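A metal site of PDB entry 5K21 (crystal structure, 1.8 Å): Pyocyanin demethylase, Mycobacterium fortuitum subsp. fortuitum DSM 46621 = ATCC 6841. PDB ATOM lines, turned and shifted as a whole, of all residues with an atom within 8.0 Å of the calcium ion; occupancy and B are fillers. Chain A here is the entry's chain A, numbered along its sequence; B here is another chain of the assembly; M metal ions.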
ATOM      1  N   HIS A  27     -21.414  27.569  23.320  1.00  0.00           N
ATOM      2  CA  HIS A  27     -22.085  26.904  22.212  1.00  0.00           C
ATOM      3  C   HIS A  27     -23.412  27.586  21.959  1.00  0.00           C
ATOM      4  O   HIS A  27     -24.319  27.535  22.793  1.00  0.00           O
ATOM      5  CB  HIS A  27     -22.333  25.435  22.499  1.00  0.00           C
ATOM      6  CG  HIS A  27     -21.092  24.614  22.590  1.00  0.00           C
ATOM      7  ND1 HIS A  27     -19.971  24.855  21.842  1.00  0.00           N
ATOM      8  CD2 HIS A  27     -20.798  23.550  23.383  1.00  0.00           C
ATOM      9  CE1 HIS A  27     -19.042  23.971  22.150  1.00  0.00           C
ATOM     10  NE2 HIS A  27     -19.522  23.173  23.086  1.00  0.00           N
ATOM     11  N   ASP A  28     -23.542  28.170  20.794  1.00  0.00           N
ATOM     12  CA  ASP A  28     -24.766  28.792  20.325  1.00  0.00           C
ATOM     13  C   ASP A  28     -25.414  27.837  19.334  1.00  0.00           C
ATOM     14  O   ASP A  28     -25.095  27.844  18.132  1.00  0.00           O
ATOM     15  CB  ASP A  28     -24.482  30.148  19.712  1.00  0.00           C
ATOM     16  CG  ASP A  28     -25.749  30.901  19.369  1.00  0.00           C
ATOM     17  OD1 ASP A  28     -26.836  30.292  19.459  1.00  0.00           O
ATOM     18  OD2 ASP A  28     -25.651  32.085  18.990  1.00  0.00           O
ATOM     19  N   PHE A  29     -26.302  26.998  19.845  1.00  0.00           N
ATOM     20  CA  PHE A  29     -27.070  26.081  19.024  1.00  0.00           C
ATOM     21  C   PHE A  29     -28.404  26.709  18.654  1.00  0.00           C
ATOM     22  O   PHE A  29     -28.761  27.792  19.114  1.00  0.00           O
ATOM     23  CB  PHE A  29     -27.291  24.765  19.763  1.00  0.00           C
ATOM     24  CG  PHE A  29     -26.037  24.065  20.170  1.00  0.00           C
ATOM     25  CD1 PHE A  29     -25.113  23.657  19.219  1.00  0.00           C
ATOM     26  CD2 PHE A  29     -25.811  23.762  21.492  1.00  0.00           C
ATOM     27  CE1 PHE A  29     -23.960  22.977  19.609  1.00  0.00           C
ATOM     28  CE2 PHE A  29     -24.671  23.089  21.879  1.00  0.00           C
ATOM     29  CZ  PHE A  29     -23.752  22.698  20.951  1.00  0.00           C
ATOM     30  N   GLY A  30     -29.115  26.029  17.770  1.00  0.00           N
ATOM     31  CA  GLY A  30     -30.488  26.425  17.471  1.00  0.00           C
ATOM     32  C   GLY A  30     -30.535  27.825  16.892  1.00  0.00           C
ATOM     33  O   GLY A  30     -29.756  28.198  16.016  1.00  0.00           O
ATOM     34  N   LYS A  31     -31.454  28.629  17.408  1.00  0.00           N
ATOM     35  CA  LYS A  31     -31.574  29.995  16.923  1.00  0.00           C
ATOM     36  C   LYS A  31     -30.335  30.782  17.347  1.00  0.00           C
ATOM     37  O   LYS A  31     -29.874  30.642  18.476  1.00  0.00           O
ATOM     38  CB  LYS A  31     -32.845  30.654  17.484  1.00  0.00           C
ATOM     39  N   PRO A  32     -29.774  31.602  16.465  1.00  0.00           N
ATOM     40  CA  PRO A  32     -28.627  32.424  16.868  1.00  0.00           C
ATOM     41  C   PRO A  32     -28.980  33.286  18.059  1.00  0.00           C
ATOM     42  O   PRO A  32     -30.114  33.739  18.192  1.00  0.00           O
ATOM     43  CB  PRO A  32     -28.337  33.272  15.639  1.00  0.00           C
ATOM     44  CG  PRO A  32     -28.951  32.535  14.504  1.00  0.00           C
ATOM     45  CD  PRO A  32     -30.154  31.860  15.064  1.00  0.00           C
ATOM     46  N   GLY A  33     -28.000  33.518  18.915  1.00  0.00           N
ATOM     47  CA  GLY A  33     -28.273  34.200  20.163  1.00  0.00           C
ATOM     48  C   GLY A  33     -28.750  33.232  21.213  1.00  0.00           C
ATOM     49  O   GLY A  33     -29.052  32.065  20.958  1.00  0.00           O
ATOM     50  N   MET A  34     -28.856  33.740  22.435  1.00  0.00           N
ATOM     51  CA  MET A  34     -29.232  32.894  23.560  1.00  0.00           C
ATOM     52  C   MET A  34     -30.650  32.379  23.405  1.00  0.00           C
ATOM     53  O   MET A  34     -31.591  33.147  23.164  1.00  0.00           O
ATOM     54  CB  MET A  34     -29.121  33.656  24.873  1.00  0.00           C
ATOM     55  CG  MET A  34     -27.747  33.709  25.464  1.00  0.00           C
ATOM     56  SD  MET A  34     -27.757  34.763  26.943  1.00  0.00           S
ATOM     57  CE  MET A  34     -27.889  36.326  26.144  1.00  0.00           C
ATOM     58  N   ASP A  35     -30.802  31.067  23.505  1.00  0.00           N
ATOM     59  CA  ASP A  35     -32.121  30.459  23.550  1.00  0.00           C
ATOM     60  C   ASP A  35     -31.976  29.123  24.242  1.00  0.00           C
ATOM     61  O   ASP A  35     -30.871  28.651  24.518  1.00  0.00           O
ATOM     62  CB  ASP A  35     -32.759  30.377  22.142  1.00  0.00           C
ATOM     63  CG  ASP A  35     -32.044  29.370  21.185  1.00  0.00           C
ATOM     64  OD1 ASP A  35     -30.821  29.147  21.272  1.00  0.00           O
ATOM     65  OD2 ASP A  35     -32.725  28.850  20.288  1.00  0.00           O
ATOM     66  N   VAL A  36     -33.116  28.535  24.583  1.00  0.00           N
ATOM     67  CA  VAL A  36     -33.096  27.262  25.282  1.00  0.00           C
ATOM     68  C   VAL A  36     -32.225  26.286  24.524  1.00  0.00           C
ATOM     69  O   VAL A  36     -32.348  26.136  23.302  1.00  0.00           O
ATOM     70  CB  VAL A  36     -34.528  26.740  25.455  1.00  0.00           C
ATOM     71  CG1 VAL A  36     -35.204  26.574  24.122  1.00  0.00           C
ATOM     72  CG2 VAL A  36     -34.514  25.443  26.269  1.00  0.00           C
ATOM     73  N   GLY A  37     -31.335  25.610  25.248  1.00  0.00           N
ATOM     74  CA  GLY A  37     -30.484  24.586  24.693  1.00  0.00           C
ATOM     75  C   GLY A  37     -29.048  25.012  24.430  1.00  0.00           C
ATOM     76  O   GLY A  37     -28.182  24.147  24.235  1.00  0.00           O
ATOM     77  N   ASP A  38     -28.770  26.298  24.481  1.00  0.00           N
ATOM     78  CA  ASP A  38     -27.385  26.712  24.371  1.00  0.00           C
ATOM     79  C   ASP A  38     -26.643  26.273  25.616  1.00  0.00           C
ATOM     80  O   ASP A  38     -27.240  25.925  26.645  1.00  0.00           O
ATOM     81  CB  ASP A  38     -27.281  28.230  24.180  1.00  0.00           C
ATOM     82  CG  ASP A  38     -27.839  28.708  22.846  1.00  0.00           C
ATOM     83  OD1 ASP A  38     -28.036  27.888  21.917  1.00  0.00           O
ATOM     84  OD2 ASP A  38     -28.076  29.926  22.699  1.00  0.00           O
ATOM     85  N   MET A  39     -25.328  26.237  25.532  1.00  0.00           N
ATOM     86  CA  MET A  39     -24.577  25.728  26.662  1.00  0.00           C
ATOM     87  C   MET A  39     -23.188  26.324  26.646  1.00  0.00           C
ATOM     88  O   MET A  39     -22.589  26.540  25.573  1.00  0.00           O
ATOM     89  CB  MET A  39     -24.530  24.205  26.673  1.00  0.00           C
ATOM     90  CG  MET A  39     -23.749  23.559  25.611  1.00  0.00           C
ATOM     91  SD  MET A  39     -23.956  21.785  25.896  1.00  0.00           S
ATOM     92  CE  MET A  39     -25.531  21.514  25.117  1.00  0.00           C
ATOM     93  N   PHE A  62     -28.720  26.575  29.104  1.00  0.00           N
ATOM     94  CA  PHE A  62     -29.785  27.575  29.090  1.00  0.00           C
ATOM     95  C   PHE A  62     -31.126  26.864  29.032  1.00  0.00           C
ATOM     96  O   PHE A  62     -31.458  26.217  28.043  1.00  0.00           O
ATOM     97  CB  PHE A  62     -29.633  28.541  27.908  1.00  0.00           C
ATOM     98  CG  PHE A  62     -28.482  29.455  28.046  1.00  0.00           C
ATOM     99  CD1 PHE A  62     -27.214  29.033  27.744  1.00  0.00           C
ATOM    100  CD2 PHE A  62     -28.660  30.733  28.544  1.00  0.00           C
ATOM    101  CE1 PHE A  62     -26.144  29.853  27.912  1.00  0.00           C
ATOM    102  CE2 PHE A  62     -27.580  31.579  28.700  1.00  0.00           C
ATOM    103  CZ  PHE A  62     -26.322  31.145  28.381  1.00  0.00           C
ATOM    104  N   VAL A  65     -35.070  31.217  28.203  1.00  0.00           N
ATOM    105  CA  VAL A  65     -34.550  32.533  27.830  1.00  0.00           C
ATOM    106  C   VAL A  65     -35.742  33.371  27.428  1.00  0.00           C
ATOM    107  O   VAL A  65     -36.509  32.969  26.545  1.00  0.00           O
ATOM    108  CB  VAL A  65     -33.507  32.469  26.702  1.00  0.00           C
ATOM    109  CG1 VAL A  65     -32.974  33.888  26.404  1.00  0.00           C
ATOM    110  CG2 VAL A  65     -32.412  31.497  27.073  1.00  0.00           C
ATOM    111  N   HIS B  27     -31.686  18.545  21.129  1.00  0.00           N
ATOM    112  CA  HIS B  27     -30.478  18.569  20.309  1.00  0.00           C
ATOM    113  C   HIS B  27     -30.316  17.208  19.637  1.00  0.00           C
ATOM    114  O   HIS B  27     -30.089  16.187  20.310  1.00  0.00           O
ATOM    115  CB  HIS B  27     -29.252  18.873  21.166  1.00  0.00           C
ATOM    116  CG  HIS B  27     -29.212  20.275  21.690  1.00  0.00           C
ATOM    117  ND1 HIS B  27     -29.636  21.362  20.958  1.00  0.00           N
ATOM    118  CD2 HIS B  27     -28.774  20.768  22.876  1.00  0.00           C
ATOM    119  CE1 HIS B  27     -29.483  22.464  21.680  1.00  0.00           C
ATOM    120  NE2 HIS B  27     -28.945  22.124  22.838  1.00  0.00           N
HETATM  121 CA    CA M   1     -28.833  29.795  20.343  1.00  0.00          CA
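O of Asp 38 sits at hydrogen-bond distance from N of Phe 62 (2.9 Å).
The calcium ion is bound by the side-chain carboxylate (OD1) of Asp 28, the side-chain carboxylate (OD1) of Asp 35, the backbone carbonyl oxygen (O) of Lys 31, the backbone carbonyl oxygen (O) of Phe 29, the backbone carbonyl oxygen (O) of Gly 33, the side-chain carboxylate (OD2) of Asp 38 and the side-chain carboxylate (OD1) of Asp 38.
The calcium ion has seven donor atoms within binding distance.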
